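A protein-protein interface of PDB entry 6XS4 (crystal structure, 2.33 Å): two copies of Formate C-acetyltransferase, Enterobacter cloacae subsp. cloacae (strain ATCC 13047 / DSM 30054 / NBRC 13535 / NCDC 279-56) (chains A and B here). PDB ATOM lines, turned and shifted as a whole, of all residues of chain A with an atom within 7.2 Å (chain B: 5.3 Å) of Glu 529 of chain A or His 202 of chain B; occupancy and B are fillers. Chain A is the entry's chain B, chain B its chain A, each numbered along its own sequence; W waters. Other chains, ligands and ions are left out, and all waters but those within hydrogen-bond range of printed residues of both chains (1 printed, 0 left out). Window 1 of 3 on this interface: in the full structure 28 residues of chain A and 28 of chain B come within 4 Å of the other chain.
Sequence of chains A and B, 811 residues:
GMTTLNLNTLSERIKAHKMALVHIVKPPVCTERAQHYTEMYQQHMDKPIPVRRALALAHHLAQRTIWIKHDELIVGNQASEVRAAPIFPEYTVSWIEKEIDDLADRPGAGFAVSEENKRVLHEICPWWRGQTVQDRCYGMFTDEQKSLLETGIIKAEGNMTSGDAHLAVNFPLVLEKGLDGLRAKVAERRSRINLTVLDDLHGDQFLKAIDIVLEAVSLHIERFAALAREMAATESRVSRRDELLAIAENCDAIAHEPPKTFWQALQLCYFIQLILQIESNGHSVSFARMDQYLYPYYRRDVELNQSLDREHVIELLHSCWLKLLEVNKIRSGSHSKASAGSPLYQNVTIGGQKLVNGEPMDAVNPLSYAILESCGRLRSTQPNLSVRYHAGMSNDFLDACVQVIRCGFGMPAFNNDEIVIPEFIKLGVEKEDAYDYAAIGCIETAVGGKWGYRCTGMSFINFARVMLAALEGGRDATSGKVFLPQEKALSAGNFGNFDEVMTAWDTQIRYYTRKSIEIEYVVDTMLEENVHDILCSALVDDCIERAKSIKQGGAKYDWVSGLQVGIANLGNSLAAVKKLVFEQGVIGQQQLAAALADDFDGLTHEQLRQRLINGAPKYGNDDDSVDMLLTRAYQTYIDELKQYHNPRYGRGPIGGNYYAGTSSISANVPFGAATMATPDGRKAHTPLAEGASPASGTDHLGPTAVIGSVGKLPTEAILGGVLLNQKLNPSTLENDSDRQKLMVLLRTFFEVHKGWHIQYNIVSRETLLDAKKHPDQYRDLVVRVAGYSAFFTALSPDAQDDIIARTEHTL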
ATOM      1  N   ILE A  49      27.097  -3.069  15.146  1.00  0.00           N
ATOM      2  CA  ILE A  49      27.193  -4.065  14.079  1.00  0.00           C
ATOM      3  C   ILE A  49      27.618  -3.447  12.753  1.00  0.00           C
ATOM      4  O   ILE A  49      28.522  -3.995  12.106  1.00  0.00           O
ATOM      5  CB  ILE A  49      25.864  -4.851  13.974  1.00  0.00           C
ATOM      6  CG1 ILE A  49      25.647  -5.669  15.250  1.00  0.00           C
ATOM      7  CG2 ILE A  49      25.886  -5.749  12.747  1.00  0.00           C
ATOM      8  CD1 ILE A  49      24.265  -6.291  15.363  1.00  0.00           C
ATOM      9  N   PRO A  50      27.047  -2.326  12.300  1.00  0.00           N
ATOM     10  CA  PRO A  50      27.509  -1.752  11.022  1.00  0.00           C
ATOM     11  C   PRO A  50      28.993  -1.433  11.010  1.00  0.00           C
ATOM     12  O   PRO A  50      29.680  -1.736  10.025  1.00  0.00           O
ATOM     13  CB  PRO A  50      26.654  -0.483  10.874  1.00  0.00           C
ATOM     14  CG  PRO A  50      25.472  -0.700  11.762  1.00  0.00           C
ATOM     15  CD  PRO A  50      25.966  -1.530  12.908  1.00  0.00           C
ATOM     16  N   ARG A  53      30.972  -4.643  10.937  1.00  0.00           N
ATOM     17  CA  ARG A  53      30.998  -5.238   9.605  1.00  0.00           C
ATOM     18  C   ARG A  53      31.866  -4.435   8.644  1.00  0.00           C
ATOM     19  O   ARG A  53      32.498  -5.015   7.752  1.00  0.00           O
ATOM     20  CB  ARG A  53      29.574  -5.364   9.059  1.00  0.00           C
ATOM     21  CG  ARG A  53      28.725  -6.376   9.812  1.00  0.00           C
ATOM     22  CD  ARG A  53      27.361  -6.571   9.166  1.00  0.00           C
ATOM     23  NE  ARG A  53      27.462  -7.037   7.783  1.00  0.00           N
ATOM     24  CZ  ARG A  53      27.771  -8.283   7.432  1.00  0.00           C
ATOM     25  NH1 ARG A  53      28.020  -9.197   8.360  1.00  0.00           N
ATOM     26  NH2 ARG A  53      27.840  -8.615   6.149  1.00  0.00           N
ATOM     27  N   ARG A 136      18.997 -17.042  14.174  1.00  0.00           N
ATOM     28  CA  ARG A 136      18.178 -16.012  14.809  1.00  0.00           C
ATOM     29  C   ARG A 136      16.764 -15.996  14.245  1.00  0.00           C
ATOM     30  O   ARG A 136      15.809 -15.725  14.984  1.00  0.00           O
ATOM     31  CB  ARG A 136      18.841 -14.642  14.658  1.00  0.00           C
ATOM     32  CG  ARG A 136      20.168 -14.529  15.402  1.00  0.00           C
ATOM     33  CD  ARG A 136      20.350 -13.181  16.092  1.00  0.00           C
ATOM     34  NE  ARG A 136      21.179 -13.312  17.292  1.00  0.00           N
ATOM     35  CZ  ARG A 136      22.366 -12.737  17.480  1.00  0.00           C
ATOM     36  NH1 ARG A 136      22.904 -11.946  16.558  1.00  0.00           N
ATOM     37  NH2 ARG A 136      23.014 -12.947  18.616  1.00  0.00           N
ATOM     38  N   MET A 140      12.856 -16.918  16.535  1.00  0.00           N
ATOM     39  CA  MET A 140      11.671 -16.010  16.549  1.00  0.00           C
ATOM     40  C   MET A 140      10.451 -16.615  15.839  1.00  0.00           C
ATOM     41  O   MET A 140       9.327 -16.177  16.156  1.00  0.00           O
ATOM     42  CB  MET A 140      12.014 -14.664  15.901  1.00  0.00           C
ATOM     43  CG  MET A 140      11.871 -13.485  16.844  1.00  0.00           C
ATOM     44  SD  MET A 140      12.305 -11.911  16.059  1.00  0.00           S
ATOM     45  CE  MET A 140      10.834 -11.616  15.078  1.00  0.00           C
ATOM     46  N   VAL A 523      12.437 -12.813   8.640  1.00  0.00           N
ATOM     47  CA  VAL A 523      13.704 -12.961   7.929  1.00  0.00           C
ATOM     48  C   VAL A 523      14.269 -11.597   7.549  1.00  0.00           C
ATOM     49  O   VAL A 523      15.464 -11.334   7.729  1.00  0.00           O
ATOM     50  CB  VAL A 523      13.525 -13.862   6.693  1.00  0.00           C
ATOM     51  CG1 VAL A 523      14.850 -14.028   5.958  1.00  0.00           C
ATOM     52  CG2 VAL A 523      12.965 -15.223   7.096  1.00  0.00           C
ATOM     53  N   ASP A 524      13.426 -10.713   7.007  1.00  0.00           N
ATOM     54  CA  ASP A 524      13.899  -9.375   6.657  1.00  0.00           C
ATOM     55  C   ASP A 524      14.462  -8.653   7.878  1.00  0.00           C
ATOM     56  O   ASP A 524      15.509  -7.998   7.794  1.00  0.00           O
ATOM     57  CB  ASP A 524      12.770  -8.549   6.036  1.00  0.00           C
ATOM     58  CG  ASP A 524      12.543  -8.867   4.570  1.00  0.00           C
ATOM     59  OD1 ASP A 524      11.425  -8.603   4.080  1.00  0.00           O
ATOM     60  OD2 ASP A 524      13.469  -9.386   3.910  1.00  0.00           O
ATOM     61  N   THR A 525      13.782  -8.761   9.021  1.00  0.00           N
ATOM     62  CA  THR A 525      14.228  -8.047  10.213  1.00  0.00           C
ATOM     63  C   THR A 525      15.532  -8.619  10.757  1.00  0.00           C
ATOM     64  O   THR A 525      16.362  -7.867  11.285  1.00  0.00           O
ATOM     65  CB  THR A 525      13.136  -8.087  11.283  1.00  0.00           C
ATOM     66  OG1 THR A 525      11.907  -7.604  10.727  1.00  0.00           O
ATOM     67  CG2 THR A 525      13.514  -7.224  12.469  1.00  0.00           C
ATOM     68  N   MET A 526      15.734  -9.933  10.638  1.00  0.00           N
ATOM     69  CA  MET A 526      16.996 -10.525  11.066  1.00  0.00           C
ATOM     70  C   MET A 526      18.133 -10.149  10.126  1.00  0.00           C
ATOM     71  O   MET A 526      19.280 -10.013  10.566  1.00  0.00           O
ATOM     72  CB  MET A 526      16.861 -12.044  11.160  1.00  0.00           C
ATOM     73  CG  MET A 526      15.946 -12.523  12.285  1.00  0.00           C
ATOM     74  SD  MET A 526      16.436 -11.937  13.927  1.00  0.00           S
ATOM     75  CE  MET A 526      15.552 -10.381  14.022  1.00  0.00           C
ATOM     76  N   LEU A 527      17.840  -9.975   8.836  1.00  0.00           N
ATOM     77  CA  LEU A 527      18.841  -9.419   7.931  1.00  0.00           C
ATOM     78  C   LEU A 527      19.109  -7.956   8.260  1.00  0.00           C
ATOM     79  O   LEU A 527      20.262  -7.510   8.244  1.00  0.00           O
ATOM     80  CB  LEU A 527      18.377  -9.562   6.484  1.00  0.00           C
ATOM     81  CG  LEU A 527      18.224 -10.986   5.944  1.00  0.00           C
ATOM     82  CD1 LEU A 527      17.272 -10.988   4.758  1.00  0.00           C
ATOM     83  CD2 LEU A 527      19.572 -11.570   5.548  1.00  0.00           C
ATOM     84  N   GLU A 528      18.053  -7.199   8.570  1.00  0.00           N
ATOM     85  CA  GLU A 528      18.214  -5.782   8.877  1.00  0.00           C
ATOM     86  C   GLU A 528      19.143  -5.573  10.066  1.00  0.00           C
ATOM     87  O   GLU A 528      20.015  -4.697  10.035  1.00  0.00           O
ATOM     88  CB  GLU A 528      16.844  -5.156   9.151  1.00  0.00           C
ATOM     89  CG  GLU A 528      16.890  -3.682   9.545  1.00  0.00           C
ATOM     90  CD  GLU A 528      15.525  -3.131   9.913  1.00  0.00           C
ATOM     91  OE1 GLU A 528      14.526  -3.866   9.770  1.00  0.00           O
ATOM     92  OE2 GLU A 528      15.452  -1.963  10.351  1.00  0.00           O
ATOM     93  N   GLU A 529      18.979  -6.375  11.119  1.00  0.00           N
ATOM     94  CA  GLU A 529      19.665  -6.124  12.377  1.00  0.00           C
ATOM     95  C   GLU A 529      21.077  -6.692  12.427  1.00  0.00           C
ATOM     96  O   GLU A 529      21.870  -6.251  13.270  1.00  0.00           O
ATOM     97  CB  GLU A 529      18.851  -6.703  13.538  1.00  0.00           C
ATOM     98  CG  GLU A 529      17.567  -5.948  13.818  1.00  0.00           C
ATOM     99  CD  GLU A 529      16.831  -6.476  15.031  1.00  0.00           C
ATOM    100  OE1 GLU A 529      17.230  -7.534  15.565  1.00  0.00           O
ATOM    101  OE2 GLU A 529      15.852  -5.824  15.451  1.00  0.00           O
ATOM    102  N   ASN A 530      21.419  -7.642  11.557  1.00  0.00           N
ATOM    103  CA  ASN A 530      22.653  -8.401  11.715  1.00  0.00           C
ATOM    104  C   ASN A 530      23.633  -8.301  10.553  1.00  0.00           C
ATOM    105  O   ASN A 530      24.835  -8.460  10.779  1.00  0.00           O
ATOM    106  CB  ASN A 530      22.327  -9.886  11.955  1.00  0.00           C
ATOM    107  CG  ASN A 530      21.697 -10.131  13.315  1.00  0.00           C
ATOM    108  OD1 ASN A 530      22.395 -10.217  14.325  1.00  0.00           O
ATOM    109  ND2 ASN A 530      20.373 -10.237  13.347  1.00  0.00           N
ATOM    110  N   VAL A 531      23.174  -8.037   9.330  1.00  0.00           N
ATOM    111  CA  VAL A 531      24.056  -8.118   8.169  1.00  0.00           C
ATOM    112  C   VAL A 531      23.894  -6.909   7.259  1.00  0.00           C
ATOM    113  O   VAL A 531      23.543  -7.042   6.081  1.00  0.00           O
ATOM    114  CB  VAL A 531      23.806  -9.424   7.386  1.00  0.00           C
ATOM    115  CG1 VAL A 531      24.277 -10.620   8.197  1.00  0.00           C
ATOM    116  CG2 VAL A 531      22.329  -9.567   7.039  1.00  0.00           C
ATOM    117  N   HIS A 532      24.180  -5.722   7.790  1.00  0.00           N
ATOM    118  CA  HIS A 532      24.119  -4.513   6.982  1.00  0.00           C
ATOM    119  C   HIS A 532      25.083  -4.618   5.804  1.00  0.00           C
ATOM    120  O   HIS A 532      26.204  -5.115   5.942  1.00  0.00           O
ATOM    121  CB  HIS A 532      24.477  -3.284   7.825  1.00  0.00           C
ATOM    122  CG  HIS A 532      23.708  -3.171   9.106  1.00  0.00           C
ATOM    123  ND1 HIS A 532      23.824  -4.086  10.130  1.00  0.00           N
ATOM    124  CD2 HIS A 532      22.830  -2.235   9.537  1.00  0.00           C
ATOM    125  CE1 HIS A 532      23.042  -3.726  11.131  1.00  0.00           C
ATOM    126  NE2 HIS A 532      22.427  -2.606  10.796  1.00  0.00           N
ATOM    127  N   SER A 549      20.926   1.798   6.383  1.00  0.00           N
ATOM    128  CA  SER A 549      21.081   0.793   5.346  1.00  0.00           C
ATOM    129  C   SER A 549      19.824   0.690   4.484  1.00  0.00           C
ATOM    130  O   SER A 549      18.745   1.170   4.843  1.00  0.00           O
ATOM    131  CB  SER A 549      21.390  -0.573   5.964  1.00  0.00           C
ATOM    132  OG  SER A 549      20.221  -1.168   6.500  1.00  0.00           O
ATOM    133  N   LYS A 551      18.189  -1.971   4.036  1.00  0.00           N
ATOM    134  CA  LYS A 551      17.241  -2.790   4.777  1.00  0.00           C
ATOM    135  C   LYS A 551      16.536  -2.018   5.886  1.00  0.00           C
ATOM    136  O   LYS A 551      15.531  -2.509   6.411  1.00  0.00           O
ATOM    137  CB  LYS A 551      17.956  -4.007   5.366  1.00  0.00           C
ATOM    138  CG  LYS A 551      17.050  -5.211   5.594  1.00  0.00           C
ATOM    139  CD  LYS A 551      16.583  -5.811   4.277  1.00  0.00           C
ATOM    140  CE  LYS A 551      15.680  -7.017   4.496  1.00  0.00           C
ATOM    141  NZ  LYS A 551      15.325  -7.684   3.209  1.00  0.00           N
ATOM    142  N   GLN A 552      17.032  -0.836   6.251  1.00  0.00           N
ATOM    143  CA  GLN A 552      16.399   0.011   7.250  1.00  0.00           C
ATOM    144  C   GLN A 552      15.494   1.071   6.637  1.00  0.00           C
ATOM    145  O   GLN A 552      14.852   1.822   7.379  1.00  0.00           O
ATOM    146  CB  GLN A 552      17.462   0.700   8.112  1.00  0.00           C
ATOM    147  CG  GLN A 552      18.314  -0.242   8.932  1.00  0.00           C
ATOM    148  CD  GLN A 552      19.432   0.480   9.664  1.00  0.00           C
ATOM    149  OE1 GLN A 552      20.395   0.941   9.051  1.00  0.00           O
ATOM    150  NE2 GLN A 552      19.304   0.585  10.979  1.00  0.00           N
ATOM    151  N   ARG A 651       9.145   4.022   6.389  1.00  0.00           N
ATOM    152  CA  ARG A 651      10.445   4.301   6.983  1.00  0.00           C
ATOM    153  C   ARG A 651      11.394   4.995   6.013  1.00  0.00           C
ATOM    154  O   ARG A 651      12.612   4.957   6.213  1.00  0.00           O
ATOM    155  CB  ARG A 651      11.072   3.003   7.499  1.00  0.00           C
ATOM    156  CG  ARG A 651      10.207   2.260   8.514  1.00  0.00           C
ATOM    157  CD  ARG A 651      11.044   1.342   9.399  1.00  0.00           C
ATOM    158  NE  ARG A 651      11.420   0.106   8.719  1.00  0.00           N
ATOM    159  CZ  ARG A 651      12.461  -0.652   9.051  1.00  0.00           C
ATOM    160  NH1 ARG A 651      13.258  -0.302  10.052  1.00  0.00           N
ATOM    161  NH2 ARG A 651      12.712  -1.762   8.368  1.00  0.00           N
ATOM    162  N   LEU B 198       5.623  -4.262  11.522  1.00  0.00           N
ATOM    163  CA  LEU B 198       6.977  -4.314  12.066  1.00  0.00           C
ATOM    164  C   LEU B 198       6.986  -4.085  13.574  1.00  0.00           C
ATOM    165  O   LEU B 198       7.540  -4.891  14.330  1.00  0.00           O
ATOM    166  CB  LEU B 198       7.865  -3.289  11.359  1.00  0.00           C
ATOM    167  CG  LEU B 198       9.349  -3.325  11.733  1.00  0.00           C
ATOM    168  CD1 LEU B 198       9.915  -4.730  11.573  1.00  0.00           C
ATOM    169  CD2 LEU B 198      10.142  -2.329  10.896  1.00  0.00           C
ATOM    170  N   ASP B 199       6.377  -2.986  14.032  1.00  0.00           N
ATOM    171  CA  ASP B 199       6.407  -2.675  15.460  1.00  0.00           C
ATOM    172  C   ASP B 199       5.773  -3.783  16.289  1.00  0.00           C
ATOM    173  O   ASP B 199       6.161  -3.991  17.445  1.00  0.00           O
ATOM    174  CB  ASP B 199       5.694  -1.351  15.735  1.00  0.00           C
ATOM    175  CG  ASP B 199       6.434  -0.163  15.165  1.00  0.00           C
ATOM    176  OD1 ASP B 199       7.594  -0.337  14.733  1.00  0.00           O
ATOM    177  OD2 ASP B 199       5.853   0.942  15.143  1.00  0.00           O
ATOM    178  N   ASP B 200       4.792  -4.493  15.726  1.00  0.00           N
ATOM    179  CA  ASP B 200       4.150  -5.586  16.445  1.00  0.00           C
ATOM    180  C   ASP B 200       5.032  -6.827  16.502  1.00  0.00           C
ATOM    181  O   ASP B 200       4.908  -7.625  17.437  1.00  0.00           O
ATOM    182  CB  ASP B 200       2.808  -5.928  15.793  1.00  0.00           C
ATOM    183  CG  ASP B 200       1.721  -4.923  16.127  1.00  0.00           C
ATOM    184  OD1 ASP B 200       2.030  -3.904  16.779  1.00  0.00           O
ATOM    185  OD2 ASP B 200       0.555  -5.157  15.741  1.00  0.00           O
ATOM    186  N   LEU B 201       5.913  -7.014  15.517  1.00  0.00           N
ATOM    187  CA  LEU B 201       6.838  -8.141  15.563  1.00  0.00           C
ATOM    188  C   LEU B 201       7.822  -7.982  16.715  1.00  0.00           C
ATOM    189  O   LEU B 201       8.031  -8.914  17.501  1.00  0.00           O
ATOM    190  CB  LEU B 201       7.580  -8.269  14.232  1.00  0.00           C
ATOM    191  CG  LEU B 201       8.555  -9.442  14.115  1.00  0.00           C
ATOM    192  CD1 LEU B 201       7.819 -10.771  14.185  1.00  0.00           C
ATOM    193  CD2 LEU B 201       9.362  -9.343  12.827  1.00  0.00           C
ATOM    194  N   HIS B 202       8.444  -6.806  16.827  1.00  0.00           N
ATOM    195  CA  HIS B 202       9.281  -6.528  17.988  1.00  0.00           C
ATOM    196  C   HIS B 202       8.454  -6.525  19.268  1.00  0.00           C
ATOM    197  O   HIS B 202       8.888  -7.052  20.299  1.00  0.00           O
ATOM    198  CB  HIS B 202       9.990  -5.184  17.824  1.00  0.00           C
ATOM    199  CG  HIS B 202      10.977  -5.150  16.702  1.00  0.00           C
ATOM    200  ND1 HIS B 202      12.088  -5.964  16.663  1.00  0.00           N
ATOM    201  CD2 HIS B 202      11.033  -4.383  15.587  1.00  0.00           C
ATOM    202  CE1 HIS B 202      12.780  -5.709  15.566  1.00  0.00           C
ATOM    203  NE2 HIS B 202      12.162  -4.752  14.898  1.00  0.00           N
ATOM    204  N   GLY B 203       7.262  -5.926  19.221  1.00  0.00           N
ATOM    205  CA  GLY B 203       6.424  -5.879  20.406  1.00  0.00           C
ATOM    206  C   GLY B 203       6.089  -7.257  20.945  1.00  0.00           C
ATOM    207  O   GLY B 203       6.091  -7.477  22.158  1.00  0.00           O
ATOM    208  N   ASP B 204       5.805  -8.205  20.050  1.00  0.00           N
ATOM    209  CA  ASP B 204       5.418  -9.539  20.497  1.00  0.00           C
ATOM    210  C   ASP B 204       6.555 -10.230  21.234  1.00  0.00           C
ATOM    211  O   ASP B 204       6.313 -10.996  22.175  1.00  0.00           O
ATOM    212  CB  ASP B 204       4.972 -10.385  19.303  1.00  0.00           C
ATOM    213  CG  ASP B 204       4.202 -11.618  19.726  1.00  0.00           C
ATOM    214  OD1 ASP B 204       3.125 -11.458  20.337  1.00  0.00           O
ATOM    215  OD2 ASP B 204       4.674 -12.742  19.457  1.00  0.00           O
ATOM    216  N   GLN B 205       7.797  -9.984  20.818  1.00  0.00           N
ATOM    217  CA  GLN B 205       8.930 -10.570  21.521  1.00  0.00           C
ATOM    218  C   GLN B 205       9.061  -9.991  22.924  1.00  0.00           C
ATOM    219  O   GLN B 205       9.415 -10.709  23.867  1.00  0.00           O
ATOM    220  CB  GLN B 205      10.218 -10.353  20.726  1.00  0.00           C
ATOM    221  CG  GLN B 205      10.303 -11.171  19.447  1.00  0.00           C
ATOM    222  CD  GLN B 205      10.104 -12.658  19.689  1.00  0.00           C
ATOM    223  OE1 GLN B 205      10.886 -13.296  20.396  1.00  0.00           O
ATOM    224  NE2 GLN B 205       9.043 -13.214  19.116  1.00  0.00           N
ATOM    225  N   PHE B 206       8.773  -8.700  23.087  1.00  0.00           N
ATOM    226  CA  PHE B 206       8.847  -8.113  24.418  1.00  0.00           C
ATOM    227  C   PHE B 206       7.732  -8.639  25.312  1.00  0.00           C
ATOM    228  O   PHE B 206       7.940  -8.849  26.513  1.00  0.00           O
ATOM    229  CB  PHE B 206       8.792  -6.590  24.338  1.00  0.00           C
ATOM    230  CG  PHE B 206       9.233  -5.913  25.603  1.00  0.00           C
ATOM    231  CD1 PHE B 206      10.573  -5.881  25.948  1.00  0.00           C
ATOM    232  CD2 PHE B 206       8.313  -5.327  26.455  1.00  0.00           C
ATOM    233  CE1 PHE B 206      10.987  -5.272  27.111  1.00  0.00           C
ATOM    234  CE2 PHE B 206       8.721  -4.714  27.619  1.00  0.00           C
ATOM    235  CZ  PHE B 206      10.060  -4.686  27.949  1.00  0.00           C
ATOM    236  N   ALA B 547       4.039  -2.531  24.457  1.00  0.00           N
ATOM    237  CA  ALA B 547       4.873  -3.680  24.115  1.00  0.00           C
ATOM    238  C   ALA B 547       6.327  -3.260  23.906  1.00  0.00           C
ATOM    239  O   ALA B 547       6.949  -3.559  22.883  1.00  0.00           O
ATOM    240  CB  ALA B 547       4.326  -4.398  22.877  1.00  0.00           C
HETATM  241  O   HOH W   1      13.549  -3.240  12.814  1.00  0.00           O
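OE2 of Glu 528 of chain A is in salt-bridge range of NH1 of Arg 651 of chain A.
Met 140 of chain A touches Leu 201 of chain B.
Met 140 of chain A touches Gln 205 of chain B (CG to CD, 3.4 Å).
Leu 198 of chain B touches Thr 525 of chain A (CD1 to OG1, 3.6 Å).
Thr 525 of chain A touches Leu 201 of chain B.
CG2 of Thr 525 of chain A touches CE1 of His 202 of chain B, at 3.5 Å.
His 202 of chain B touches Glu 529 of chain A.
CZ of Arg 651 of chain A touches CD2 of Leu 198 of chain B (3.4 Å).
Of the printed residues of chain B, Met 140 of chain A touches Leu 201 and Gln 205.
Printed residues of chain B within 4 Å of Thr 525 of chain A: Leu 198 (3.6 Å), Leu 201 (3.7 Å) and His 202 (3.5 Å).
Glu 529 of chain A touches one residue of chain B.
His 202 of chain B touches just these residues of chain A: Thr 525 (3.5 Å) and Glu 529 (3.1 Å).
The nearest printed residue of chain A that does not touch His 202 of chain B is Met 526 of chain A (5.6 Å).
Of the 10 printed residues of chain B, 4 touch a printed residue of chain A.
Printed residues of chain B that touch a printed residue of chain A: Leu 198, Leu 201, His 202 and Gln 205.
Among the printed residues, 7 pairs touch across the chains.
Among the printed residues, no Asp or Glu carboxylate lies within 4 Å of a Lys or Arg side-chain nitrogen of the other chain.
No position is printed for both chains.
Of the 7 pairs that touch across the chains among the printed residues, none has its exchanged pair printed and touching as well.
Water W1 bridges a ring nitrogen (NE2) of His 202 of chain B and the side-chain carboxylate (OE1) of Glu 528 of chain A.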
